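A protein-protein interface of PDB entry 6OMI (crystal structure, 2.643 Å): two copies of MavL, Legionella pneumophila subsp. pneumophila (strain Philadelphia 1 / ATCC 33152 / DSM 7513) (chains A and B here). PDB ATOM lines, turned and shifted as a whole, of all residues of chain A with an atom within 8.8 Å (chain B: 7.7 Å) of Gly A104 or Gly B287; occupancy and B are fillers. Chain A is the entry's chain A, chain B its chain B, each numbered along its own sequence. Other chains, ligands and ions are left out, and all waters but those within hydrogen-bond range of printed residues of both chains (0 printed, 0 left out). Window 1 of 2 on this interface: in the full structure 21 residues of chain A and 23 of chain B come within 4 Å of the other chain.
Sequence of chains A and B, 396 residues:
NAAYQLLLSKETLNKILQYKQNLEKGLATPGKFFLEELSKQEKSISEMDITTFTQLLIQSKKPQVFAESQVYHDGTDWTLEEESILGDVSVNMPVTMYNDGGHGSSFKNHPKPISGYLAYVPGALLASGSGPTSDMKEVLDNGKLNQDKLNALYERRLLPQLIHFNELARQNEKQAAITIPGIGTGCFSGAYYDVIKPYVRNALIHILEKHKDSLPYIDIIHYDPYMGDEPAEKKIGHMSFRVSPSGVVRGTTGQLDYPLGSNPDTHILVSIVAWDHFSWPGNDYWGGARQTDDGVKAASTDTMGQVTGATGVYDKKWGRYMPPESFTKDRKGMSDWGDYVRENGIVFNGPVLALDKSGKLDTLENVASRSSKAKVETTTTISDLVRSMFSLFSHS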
ATOM      1  N   ASN A  99      12.275 -13.980  29.051  1.00  0.00           N
ATOM      2  CA  ASN A  99      11.250 -13.751  28.043  1.00  0.00           C
ATOM      3  C   ASN A  99      11.790 -14.172  26.682  1.00  0.00           C
ATOM      4  O   ASN A  99      12.938 -14.608  26.552  1.00  0.00           O
ATOM      5  CB  ASN A  99      10.789 -12.287  28.031  1.00  0.00           C
ATOM      6  CG  ASN A  99      11.915 -11.320  27.723  1.00  0.00           C
ATOM      7  OD1 ASN A  99      12.372 -11.221  26.584  1.00  0.00           O
ATOM      8  ND2 ASN A  99      12.362 -10.594  28.740  1.00  0.00           N
ATOM      9  N   ASP A 100      10.946 -14.037  25.657  1.00  0.00           N
ATOM     10  CA  ASP A 100      11.272 -14.500  24.313  1.00  0.00           C
ATOM     11  C   ASP A 100      12.283 -13.614  23.596  1.00  0.00           C
ATOM     12  O   ASP A 100      12.698 -13.963  22.485  1.00  0.00           O
ATOM     13  CB  ASP A 100       9.996 -14.597  23.473  1.00  0.00           C
ATOM     14  CG  ASP A 100       9.329 -13.250  23.271  1.00  0.00           C
ATOM     15  OD1 ASP A 100       9.396 -12.407  24.189  1.00  0.00           O
ATOM     16  OD2 ASP A 100       8.739 -13.033  22.191  1.00  0.00           O
ATOM     17  N   GLY A 101      12.687 -12.491  24.186  1.00  0.00           N
ATOM     18  CA  GLY A 101      13.644 -11.617  23.537  1.00  0.00           C
ATOM     19  C   GLY A 101      13.052 -10.626  22.565  1.00  0.00           C
ATOM     20  O   GLY A 101      13.775 -10.108  21.709  1.00  0.00           O
ATOM     21  N   GLY A 102      11.756 -10.341  22.667  1.00  0.00           N
ATOM     22  CA  GLY A 102      11.146  -9.373  21.779  1.00  0.00           C
ATOM     23  C   GLY A 102      11.550  -7.951  22.122  1.00  0.00           C
ATOM     24  O   GLY A 102      11.787  -7.603  23.278  1.00  0.00           O
ATOM     25  N   HIS A 103      11.633  -7.118  21.088  1.00  0.00           N
ATOM     26  CA  HIS A 103      12.022  -5.729  21.273  1.00  0.00           C
ATOM     27  C   HIS A 103      10.825  -4.883  21.687  1.00  0.00           C
ATOM     28  O   HIS A 103       9.671  -5.210  21.393  1.00  0.00           O
ATOM     29  CB  HIS A 103      12.641  -5.160  19.994  1.00  0.00           C
ATOM     30  CG  HIS A 103      13.939  -5.801  19.609  1.00  0.00           C
ATOM     31  ND1 HIS A 103      14.284  -7.081  19.986  1.00  0.00           N
ATOM     32  CD2 HIS A 103      14.980  -5.332  18.880  1.00  0.00           C
ATOM     33  CE1 HIS A 103      15.479  -7.373  19.505  1.00  0.00           C
ATOM     34  NE2 HIS A 103      15.922  -6.329  18.829  1.00  0.00           N
ATOM     35  N   GLY A 104      11.117  -3.778  22.369  1.00  0.00           N
ATOM     36  CA  GLY A 104      10.067  -2.892  22.841  1.00  0.00           C
ATOM     37  C   GLY A 104       9.170  -3.580  23.847  1.00  0.00           C
ATOM     38  O   GLY A 104       9.630  -4.286  24.752  1.00  0.00           O
ATOM     39  N   SER A 105       7.864  -3.375  23.692  1.00  0.00           N
ATOM     40  CA  SER A 105       6.868  -4.011  24.544  1.00  0.00           C
ATOM     41  C   SER A 105       6.384  -5.341  23.986  1.00  0.00           C
ATOM     42  O   SER A 105       5.483  -5.951  24.570  1.00  0.00           O
ATOM     43  CB  SER A 105       5.670  -3.079  24.746  1.00  0.00           C
ATOM     44  OG  SER A 105       5.182  -2.599  23.507  1.00  0.00           O
ATOM     45  N   SER A 106       6.963  -5.802  22.879  1.00  0.00           N
ATOM     46  CA  SER A 106       6.532  -7.027  22.220  1.00  0.00           C
ATOM     47  C   SER A 106       7.047  -8.287  22.900  1.00  0.00           C
ATOM     48  O   SER A 106       6.774  -9.389  22.410  1.00  0.00           O
ATOM     49  CB  SER A 106       6.978  -7.013  20.756  1.00  0.00           C
ATOM     50  OG  SER A 106       8.387  -7.105  20.655  1.00  0.00           O
ATOM     51  N   PHE A 107       7.783  -8.162  24.001  1.00  0.00           N
ATOM     52  CA  PHE A 107       8.306  -9.331  24.690  1.00  0.00           C
ATOM     53  C   PHE A 107       7.196 -10.026  25.467  1.00  0.00           C
ATOM     54  O   PHE A 107       6.310  -9.377  26.031  1.00  0.00           O
ATOM     55  CB  PHE A 107       9.447  -8.938  25.633  1.00  0.00           C
ATOM     56  CG  PHE A 107       9.018  -8.078  26.793  1.00  0.00           C
ATOM     57  CD1 PHE A 107       8.974  -6.699  26.669  1.00  0.00           C
ATOM     58  CD2 PHE A 107       8.673  -8.645  28.012  1.00  0.00           C
ATOM     59  CE1 PHE A 107       8.584  -5.901  27.730  1.00  0.00           C
ATOM     60  CE2 PHE A 107       8.280  -7.852  29.077  1.00  0.00           C
ATOM     61  CZ  PHE A 107       8.237  -6.478  28.936  1.00  0.00           C
ATOM     62  N   LYS A 108       7.247 -11.355  25.489  1.00  0.00           N
ATOM     63  CA  LYS A 108       6.298 -12.173  26.231  1.00  0.00           C
ATOM     64  C   LYS A 108       7.062 -12.923  27.310  1.00  0.00           C
ATOM     65  O   LYS A 108       7.981 -13.691  27.004  1.00  0.00           O
ATOM     66  CB  LYS A 108       5.564 -13.148  25.306  1.00  0.00           C
ATOM     67  CG  LYS A 108       4.795 -12.476  24.181  1.00  0.00           C
ATOM     68  N   ARG A 290      17.421  -1.149  26.837  1.00  0.00           N
ATOM     69  CA  ARG A 290      17.114  -2.485  26.324  1.00  0.00           C
ATOM     70  C   ARG A 290      16.953  -2.418  24.805  1.00  0.00           C
ATOM     71  O   ARG A 290      15.873  -2.593  24.243  1.00  0.00           O
ATOM     72  CB  ARG A 290      15.860  -3.033  26.997  1.00  0.00           C
ATOM     73  CG  ARG A 290      15.515  -4.466  26.618  1.00  0.00           C
ATOM     74  CD  ARG A 290      14.507  -5.060  27.584  1.00  0.00           C
ATOM     75  NE  ARG A 290      14.102  -6.407  27.193  1.00  0.00           N
ATOM     76  CZ  ARG A 290      13.255  -6.680  26.207  1.00  0.00           C
ATOM     77  NH1 ARG A 290      12.712  -5.697  25.501  1.00  0.00           N
ATOM     78  NH2 ARG A 290      12.949  -7.939  25.927  1.00  0.00           N
ATOM     79  N   GLN A 291      18.064  -2.113  24.141  1.00  0.00           N
ATOM     80  CA  GLN A 291      18.049  -1.857  22.713  1.00  0.00           C
ATOM     81  C   GLN A 291      18.993  -2.800  21.984  1.00  0.00           C
ATOM     82  O   GLN A 291      19.943  -3.329  22.567  1.00  0.00           O
ATOM     83  CB  GLN A 291      18.450  -0.414  22.453  1.00  0.00           C
ATOM     84  CG  GLN A 291      17.583   0.569  23.213  1.00  0.00           C
ATOM     85  CD  GLN A 291      16.092   0.247  23.198  1.00  0.00           C
ATOM     86  OE1 GLN A 291      15.417   0.372  24.220  1.00  0.00           O
ATOM     87  NE2 GLN A 291      15.567  -0.129  22.034  1.00  0.00           N
ATOM     88  N   THR A 292      18.723  -2.993  20.689  1.00  0.00           N
ATOM     89  CA  THR A 292      19.544  -3.816  19.804  1.00  0.00           C
ATOM     90  C   THR A 292      19.519  -5.274  20.247  1.00  0.00           C
ATOM     91  O   THR A 292      19.092  -5.590  21.362  1.00  0.00           O
ATOM     92  CB  THR A 292      20.991  -3.309  19.725  1.00  0.00           C
ATOM     93  OG1 THR A 292      21.635  -3.455  20.998  1.00  0.00           O
ATOM     94  CG2 THR A 292      21.026  -1.848  19.306  1.00  0.00           C
ATOM     95  N   VAL A 296      18.943  -6.194  24.169  1.00  0.00           N
ATOM     96  CA  VAL A 296      17.686  -6.884  24.449  1.00  0.00           C
ATOM     97  C   VAL A 296      17.955  -8.294  24.956  1.00  0.00           C
ATOM     98  O   VAL A 296      17.351  -8.743  25.938  1.00  0.00           O
ATOM     99  CB  VAL A 296      16.788  -6.897  23.199  1.00  0.00           C
ATOM    100  CG1 VAL A 296      15.626  -7.859  23.387  1.00  0.00           C
ATOM    101  CG2 VAL A 296      16.274  -5.498  22.895  1.00  0.00           C
ATOM    102  N   SER A 300      17.046  -9.531  28.773  1.00  0.00           N
ATOM    103  CA  SER A 300      16.062 -10.596  28.913  1.00  0.00           C
ATOM    104  C   SER A 300      16.643 -11.869  29.514  1.00  0.00           C
ATOM    105  O   SER A 300      15.907 -12.847  29.681  1.00  0.00           O
ATOM    106  CB  SER A 300      15.432 -10.908  27.554  1.00  0.00           C
ATOM    107  OG  SER A 300      14.921  -9.734  26.947  1.00  0.00           O
ATOM    108  N   LYS A 316       9.111  -8.116  35.508  1.00  0.00           N
ATOM    109  CA  LYS A 316       8.209  -8.613  34.473  1.00  0.00           C
ATOM    110  C   LYS A 316       7.504  -7.475  33.743  1.00  0.00           C
ATOM    111  O   LYS A 316       7.267  -7.565  32.533  1.00  0.00           O
ATOM    112  CB  LYS A 316       7.180  -9.564  35.084  1.00  0.00           C
ATOM    113  CG  LYS A 316       7.783 -10.759  35.799  1.00  0.00           C
ATOM    114  CD  LYS A 316       6.703 -11.629  36.420  1.00  0.00           C
ATOM    115  N   LYS A 317       7.159  -6.402  34.458  1.00  0.00           N
ATOM    116  CA  LYS A 317       6.508  -5.261  33.825  1.00  0.00           C
ATOM    117  C   LYS A 317       7.432  -4.522  32.868  1.00  0.00           C
ATOM    118  O   LYS A 317       6.951  -3.745  32.036  1.00  0.00           O
ATOM    119  CB  LYS A 317       5.982  -4.295  34.888  1.00  0.00           C
ATOM    120  N   TRP A 318       8.744  -4.740  32.969  1.00  0.00           N
ATOM    121  CA  TRP A 318       9.708  -4.096  32.093  1.00  0.00           C
ATOM    122  C   TRP A 318      10.547  -5.066  31.276  1.00  0.00           C
ATOM    123  O   TRP A 318      11.220  -4.627  30.336  1.00  0.00           O
ATOM    124  CB  TRP A 318      10.647  -3.192  32.908  1.00  0.00           C
ATOM    125  CG  TRP A 318       9.939  -2.079  33.608  1.00  0.00           C
ATOM    126  CD1 TRP A 318       9.406  -2.106  34.864  1.00  0.00           C
ATOM    127  CD2 TRP A 318       9.694  -0.765  33.095  1.00  0.00           C
ATOM    128  NE1 TRP A 318       8.838  -0.890  35.162  1.00  0.00           N
ATOM    129  CE2 TRP A 318       9.002  -0.050  34.091  1.00  0.00           C
ATOM    130  CE3 TRP A 318       9.991  -0.126  31.888  1.00  0.00           C
ATOM    131  CZ2 TRP A 318       8.602   1.273  33.919  1.00  0.00           C
ATOM    132  CZ3 TRP A 318       9.594   1.186  31.718  1.00  0.00           C
ATOM    133  CH2 TRP A 318       8.907   1.872  32.728  1.00  0.00           C
ATOM    134  N   GLY A 319      10.526  -6.357  31.591  1.00  0.00           N
ATOM    135  CA  GLY A 319      11.282  -7.319  30.807  1.00  0.00           C
ATOM    136  C   GLY A 319      12.779  -7.105  30.848  1.00  0.00           C
ATOM    137  O   GLY A 319      13.441  -7.174  29.805  1.00  0.00           O
ATOM    138  N   ARG A 320      13.333  -6.843  32.031  1.00  0.00           N
ATOM    139  CA  ARG A 320      14.752  -6.542  32.166  1.00  0.00           C
ATOM    140  C   ARG A 320      15.296  -7.139  33.454  1.00  0.00           C
ATOM    141  O   ARG A 320      14.601  -7.180  34.473  1.00  0.00           O
ATOM    142  CB  ARG A 320      15.010  -5.026  32.190  1.00  0.00           C
ATOM    143  CG  ARG A 320      14.434  -4.240  31.026  1.00  0.00           C
ATOM    144  CD  ARG A 320      14.095  -2.819  31.446  1.00  0.00           C
ATOM    145  NE  ARG A 320      13.640  -2.008  30.321  1.00  0.00           N
ATOM    146  CZ  ARG A 320      14.398  -1.118  29.689  1.00  0.00           C
ATOM    147  NH1 ARG A 320      15.652  -0.922  30.072  1.00  0.00           N
ATOM    148  NH2 ARG A 320      13.902  -0.423  28.673  1.00  0.00           N
ATOM    149  N   PRO B  63       1.314   5.040  14.331  1.00  0.00           N
ATOM    150  CA  PRO B  63       2.053   5.514  15.515  1.00  0.00           C
ATOM    151  C   PRO B  63       3.532   5.164  15.508  1.00  0.00           C
ATOM    152  O   PRO B  63       4.358   5.991  15.914  1.00  0.00           O
ATOM    153  CB  PRO B  63       1.315   4.833  16.677  1.00  0.00           C
ATOM    154  CG  PRO B  63      -0.073   4.630  16.164  1.00  0.00           C
ATOM    155  CD  PRO B  63       0.087   4.308  14.703  1.00  0.00           C
ATOM    156  N   GLN B  64       3.896   3.961  15.064  1.00  0.00           N
ATOM    157  CA  GLN B  64       5.283   3.506  15.089  1.00  0.00           C
ATOM    158  C   GLN B  64       5.606   2.846  13.756  1.00  0.00           C
ATOM    159  O   GLN B  64       5.044   1.797  13.426  1.00  0.00           O
ATOM    160  CB  GLN B  64       5.524   2.539  16.250  1.00  0.00           C
ATOM    161  CG  GLN B  64       6.962   2.050  16.366  1.00  0.00           C
ATOM    162  CD  GLN B  64       7.206   0.758  15.615  1.00  0.00           C
ATOM    163  OE1 GLN B  64       8.120   0.666  14.794  1.00  0.00           O
ATOM    164  NE2 GLN B  64       6.394  -0.253  15.895  1.00  0.00           N
ATOM    165  N   VAL B  65       6.511   3.459  12.993  1.00  0.00           N
ATOM    166  CA  VAL B  65       6.930   2.955  11.689  1.00  0.00           C
ATOM    167  C   VAL B  65       8.444   3.079  11.585  1.00  0.00           C
ATOM    168  O   VAL B  65       9.018   4.106  11.959  1.00  0.00           O
ATOM    169  CB  VAL B  65       6.244   3.718  10.532  1.00  0.00           C
ATOM    170  CG1 VAL B  65       6.745   3.216   9.185  1.00  0.00           C
ATOM    171  CG2 VAL B  65       4.734   3.585  10.618  1.00  0.00           C
ATOM    172  N   GLY B 282       6.836  10.852  18.064  1.00  0.00           N
ATOM    173  CA  GLY B 282       7.258   9.916  19.094  1.00  0.00           C
ATOM    174  C   GLY B 282       7.714   8.576  18.551  1.00  0.00           C
ATOM    175  O   GLY B 282       8.551   7.916  19.174  1.00  0.00           O
ATOM    176  N   ASN B 283       7.186   8.175  17.390  1.00  0.00           N
ATOM    177  CA  ASN B 283       7.537   6.948  16.676  1.00  0.00           C
ATOM    178  C   ASN B 283       7.888   5.777  17.588  1.00  0.00           C
ATOM    179  O   ASN B 283       7.005   5.028  18.020  1.00  0.00           O
ATOM    180  CB  ASN B 283       8.700   7.208  15.714  1.00  0.00           C
ATOM    181  CG  ASN B 283       8.785   6.169  14.605  1.00  0.00           C
ATOM    182  OD1 ASN B 283       8.276   5.055  14.739  1.00  0.00           O
ATOM    183  ND2 ASN B 283       9.433   6.531  13.504  1.00  0.00           N
ATOM    184  N   ASP B 284       9.181   5.623  17.888  1.00  0.00           N
ATOM    185  CA  ASP B 284       9.643   4.425  18.580  1.00  0.00           C
ATOM    186  C   ASP B 284       9.027   4.297  19.966  1.00  0.00           C
ATOM    187  O   ASP B 284       8.728   3.182  20.409  1.00  0.00           O
ATOM    188  CB  ASP B 284      11.169   4.430  18.681  1.00  0.00           C
ATOM    189  CG  ASP B 284      11.847   4.469  17.324  1.00  0.00           C
ATOM    190  OD1 ASP B 284      11.622   5.441  16.573  1.00  0.00           O
ATOM    191  OD2 ASP B 284      12.616   3.535  17.014  1.00  0.00           O
ATOM    192  N   TYR B 285       8.803   5.419  20.658  1.00  0.00           N
ATOM    193  CA  TYR B 285       8.208   5.343  21.988  1.00  0.00           C
ATOM    194  C   TYR B 285       6.744   4.932  21.942  1.00  0.00           C
ATOM    195  O   TYR B 285       6.207   4.486  22.962  1.00  0.00           O
ATOM    196  CB  TYR B 285       8.347   6.673  22.727  1.00  0.00           C
ATOM    197  CG  TYR B 285       7.893   6.587  24.169  1.00  0.00           C
ATOM    198  CD1 TYR B 285       8.390   5.602  25.011  1.00  0.00           C
ATOM    199  CD2 TYR B 285       6.959   7.478  24.685  1.00  0.00           C
ATOM    200  CE1 TYR B 285       7.974   5.508  26.326  1.00  0.00           C
ATOM    201  CE2 TYR B 285       6.538   7.392  26.001  1.00  0.00           C
ATOM    202  CZ  TYR B 285       7.050   6.407  26.817  1.00  0.00           C
ATOM    203  OH  TYR B 285       6.636   6.316  28.128  1.00  0.00           O
ATOM    204  N   TRP B 286       6.084   5.068  20.790  1.00  0.00           N
ATOM    205  CA  TRP B 286       4.754   4.492  20.651  1.00  0.00           C
ATOM    206  C   TRP B 286       4.788   2.975  20.761  1.00  0.00           C
ATOM    207  O   TRP B 286       3.759   2.361  21.066  1.00  0.00           O
ATOM    208  CB  TRP B 286       4.121   4.916  19.326  1.00  0.00           C
ATOM    209  CG  TRP B 286       3.762   6.369  19.273  1.00  0.00           C
ATOM    210  CD1 TRP B 286       4.436   7.361  18.623  1.00  0.00           C
ATOM    211  CD2 TRP B 286       2.648   6.996  19.915  1.00  0.00           C
ATOM    212  NE1 TRP B 286       3.802   8.566  18.810  1.00  0.00           N
ATOM    213  CE2 TRP B 286       2.701   8.368  19.601  1.00  0.00           C
ATOM    214  CE3 TRP B 286       1.606   6.529  20.719  1.00  0.00           C
ATOM    215  CZ2 TRP B 286       1.755   9.276  20.069  1.00  0.00           C
ATOM    216  CZ3 TRP B 286       0.670   7.432  21.182  1.00  0.00           C
ATOM    217  CH2 TRP B 286       0.748   8.786  20.854  1.00  0.00           C
ATOM    218  N   GLY B 287       5.943   2.362  20.520  1.00  0.00           N
ATOM    219  CA  GLY B 287       6.166   0.960  20.786  1.00  0.00           C
ATOM    220  C   GLY B 287       6.789   0.676  22.134  1.00  0.00           C
ATOM    221  O   GLY B 287       7.160  -0.472  22.404  1.00  0.00           O
ATOM    222  N   GLY B 288       6.914   1.686  22.992  1.00  0.00           N
ATOM    223  CA  GLY B 288       7.426   1.507  24.333  1.00  0.00           C
ATOM    224  C   GLY B 288       8.929   1.580  24.482  1.00  0.00           C
ATOM    225  O   GLY B 288       9.439   1.289  25.570  1.00  0.00           O
ATOM    226  N   ALA B 289       9.654   1.967  23.436  1.00  0.00           N
ATOM    227  CA  ALA B 289      11.110   2.039  23.466  1.00  0.00           C
ATOM    228  C   ALA B 289      11.534   3.501  23.464  1.00  0.00           C
ATOM    229  O   ALA B 289      11.160   4.259  22.564  1.00  0.00           O
ATOM    230  CB  ALA B 289      11.721   1.297  22.277  1.00  0.00           C
ATOM    231  N   ARG B 290      12.319   3.891  24.470  1.00  0.00           N
ATOM    232  CA  ARG B 290      12.818   5.262  24.600  1.00  0.00           C
ATOM    233  C   ARG B 290      14.103   5.427  23.781  1.00  0.00           C
ATOM    234  O   ARG B 290      15.206   5.598  24.303  1.00  0.00           O
ATOM    235  CB  ARG B 290      13.021   5.604  26.071  1.00  0.00           C
ATOM    236  CG  ARG B 290      13.436   7.045  26.352  1.00  0.00           C
ATOM    237  CD  ARG B 290      13.223   7.398  27.821  1.00  0.00           C
ATOM    238  NE  ARG B 290      13.702   8.739  28.142  1.00  0.00           N
ATOM    239  CZ  ARG B 290      14.985   9.057  28.299  1.00  0.00           C
ATOM    240  NH1 ARG B 290      15.924   8.129  28.166  1.00  0.00           N
ATOM    241  NH2 ARG B 290      15.330  10.303  28.590  1.00  0.00           N
ATOM    242  N   MET B 304       2.670  12.375  24.192  1.00  0.00           N
ATOM    243  CA  MET B 304       1.585  11.414  24.080  1.00  0.00           C
ATOM    244  C   MET B 304       0.307  11.971  24.691  1.00  0.00           C
ATOM    245  O   MET B 304      -0.781  11.773  24.155  1.00  0.00           O
ATOM    246  CB  MET B 304       1.973  10.095  24.748  1.00  0.00           C
ATOM    247  CG  MET B 304       2.764   9.156  23.848  1.00  0.00           C
ATOM    248  SD  MET B 304       4.446   9.907  23.203  1.00  0.00           S
ATOM    249  CE  MET B 304       5.016   8.433  22.062  1.00  0.00           C
ATOM    250  N   MET B 334       4.609  -5.209  29.426  1.00  0.00           N
ATOM    251  CA  MET B 334       4.670  -3.789  29.101  1.00  0.00           C
ATOM    252  C   MET B 334       3.560  -3.394  28.129  1.00  0.00           C
ATOM    253  O   MET B 334       3.326  -4.076  27.134  1.00  0.00           O
ATOM    254  CB  MET B 334       6.036  -3.433  28.509  1.00  0.00           C
ATOM    255  CG  MET B 334       6.207  -1.958  28.183  1.00  0.00           C
ATOM    256  SD  MET B 334       7.897  -1.559  27.289  1.00  0.00           S
ATOM    257  CE  MET B 334       9.130  -2.117  28.692  1.00  0.00           C
ATOM    258  N   SER B 335       2.883  -2.288  28.427  1.00  0.00           N
ATOM    259  CA  SER B 335       1.794  -1.770  27.605  1.00  0.00           C
ATOM    260  C   SER B 335       2.185  -0.379  27.123  1.00  0.00           C
ATOM    261  O   SER B 335       2.326   0.544  27.932  1.00  0.00           O
ATOM    262  CB  SER B 335       0.481  -1.739  28.388  1.00  0.00           C
ATOM    263  OG  SER B 335       0.162  -3.023  28.893  1.00  0.00           O
ATOM    264  N   ASP B 336       2.367  -0.232  25.813  1.00  0.00           N
ATOM    265  CA  ASP B 336       2.819   1.019  25.225  1.00  0.00           C
ATOM    266  C   ASP B 336       1.633   1.918  24.878  1.00  0.00           C
ATOM    267  O   ASP B 336       0.472   1.502  24.899  1.00  0.00           O
ATOM    268  CB  ASP B 336       3.674   0.752  23.982  1.00  0.00           C
ATOM    269  CG  ASP B 336       3.021  -0.220  23.013  1.00  0.00           C
ATOM    270  OD1 ASP B 336       1.777  -0.310  22.993  1.00  0.00           O
ATOM    271  OD2 ASP B 336       3.757  -0.900  22.266  1.00  0.00           O
ATOM    272  N   TRP B 337       1.943   3.177  24.560  1.00  0.00           N
ATOM    273  CA  TRP B 337       0.915   4.123  24.141  1.00  0.00           C
ATOM    274  C   TRP B 337       0.233   3.710  22.840  1.00  0.00           C
ATOM    275  O   TRP B 337      -0.892   4.154  22.573  1.00  0.00           O
ATOM    276  CB  TRP B 337       1.528   5.515  23.987  1.00  0.00           C
ATOM    277  CG  TRP B 337       1.765   6.229  25.280  1.00  0.00           C
ATOM    278  CD1 TRP B 337       2.887   6.172  26.057  1.00  0.00           C
ATOM    279  CD2 TRP B 337       0.860   7.117  25.946  1.00  0.00           C
ATOM    280  NE1 TRP B 337       2.734   6.971  27.166  1.00  0.00           N
ATOM    281  CE2 TRP B 337       1.499   7.562  27.121  1.00  0.00           C
ATOM    282  CE3 TRP B 337      -0.427   7.582  25.661  1.00  0.00           C
ATOM    283  CZ2 TRP B 337       0.893   8.448  28.009  1.00  0.00           C
ATOM    284  CZ3 TRP B 337      -1.028   8.459  26.545  1.00  0.00           C
ATOM    285  CH2 TRP B 337      -0.368   8.882  27.706  1.00  0.00           C
ATOM    286  N   GLY B 338       0.880   2.874  22.026  1.00  0.00           N
ATOM    287  CA  GLY B 338       0.222   2.365  20.835  1.00  0.00           C
ATOM    288  C   GLY B 338      -0.990   1.516  21.169  1.00  0.00           C
ATOM    289  O   GLY B 338      -2.019   1.584  20.488  1.00  0.00           O
ATOM    290  N   ASP B 339      -0.891   0.714  22.231  1.00  0.00           N
ATOM    291  CA  ASP B 339      -2.055  -0.030  22.698  1.00  0.00           C
ATOM    292  C   ASP B 339      -3.167   0.918  23.123  1.00  0.00           C
ATOM    293  O   ASP B 339      -4.353   0.634  22.911  1.00  0.00           O
ATOM    294  CB  ASP B 339      -1.660  -0.947  23.857  1.00  0.00           C
ATOM    295  CG  ASP B 339      -0.648  -2.002  23.451  1.00  0.00           C
ATOM    296  OD1 ASP B 339      -0.596  -2.355  22.253  1.00  0.00           O
ATOM    297  OD2 ASP B 339       0.102  -2.474  24.331  1.00  0.00           O
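The backbone carbonyl oxygen (O) of Gly B287 lies within hydrogen-bond range of the side-chain hydroxyl (OG) of Ser A105 (3.1 Å). The side-chain carboxylate of Asp B336 is in hydrogen-bond range of the side-chain hydroxyl of Ser A105.
OD1 of Asp B336 sits close to N of Gly B338, 3.4 Å away. OD1 of Asp B336 lies within hydrogen-bond range of N of Asp B339, at 3.0 Å. The backbone carbonyl oxygen of Gly A104 lies within hydrogen-bond range of the guanidinium group of Arg A290, 3.5 Å away.
Gly A104 touches Gly B287 (CA to O, 3.8 Å). Ser A105 touches Met B334 (CB to O, 3.5 Å). Met B334 touches Phe A107 (CB to CE1, 3.6 Å). Lys A317 touches Met B334. O of Trp A318 touches CE of Met B334 (3.7 Å).
Of chain B, only Gly B287 (3.8 Å) comes within 4 Å of Gly A104. Of chain A, only Gly A104 and Ser A105 come within 4 Å of Gly B287. Of the printed residues of chain A, Met B334 touches Ser A105, Phe A107, Lys A317 and Trp A318. Of the printed residues of chain B, Phe A107 touches Met B334. Printed residues of chain B within 4 Å of Lys A317: Met B334. Printed residues of chain B within 4 Å of Trp A318: Met B334. Of the printed residues of chain A, Asp B336 touches Ser A105 (2.5 Å). Thr A292 touches none of the printed residues of chain B.
Hydrophobic or aromatic side chains of chain A that line the printed part of chain B: Phe A107 and Trp A318. Printed residues of chain B that touch a printed residue of chain A: Gly B287, Met B334 and Asp B336. Along chain B the printed residues that touch a printed residue of chain A span positions 287 to 336. Among the printed residues, 7 pairs touch across the chains. Among the printed residues, no Asp or Glu carboxylate lies within 4 Å of a Lys or Arg side-chain nitrogen of the other chain.
Position printed for both chains: 290. Of the 7 pairs that touch across the chains among the printed residues, none has its exchanged pair printed and touching as well.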
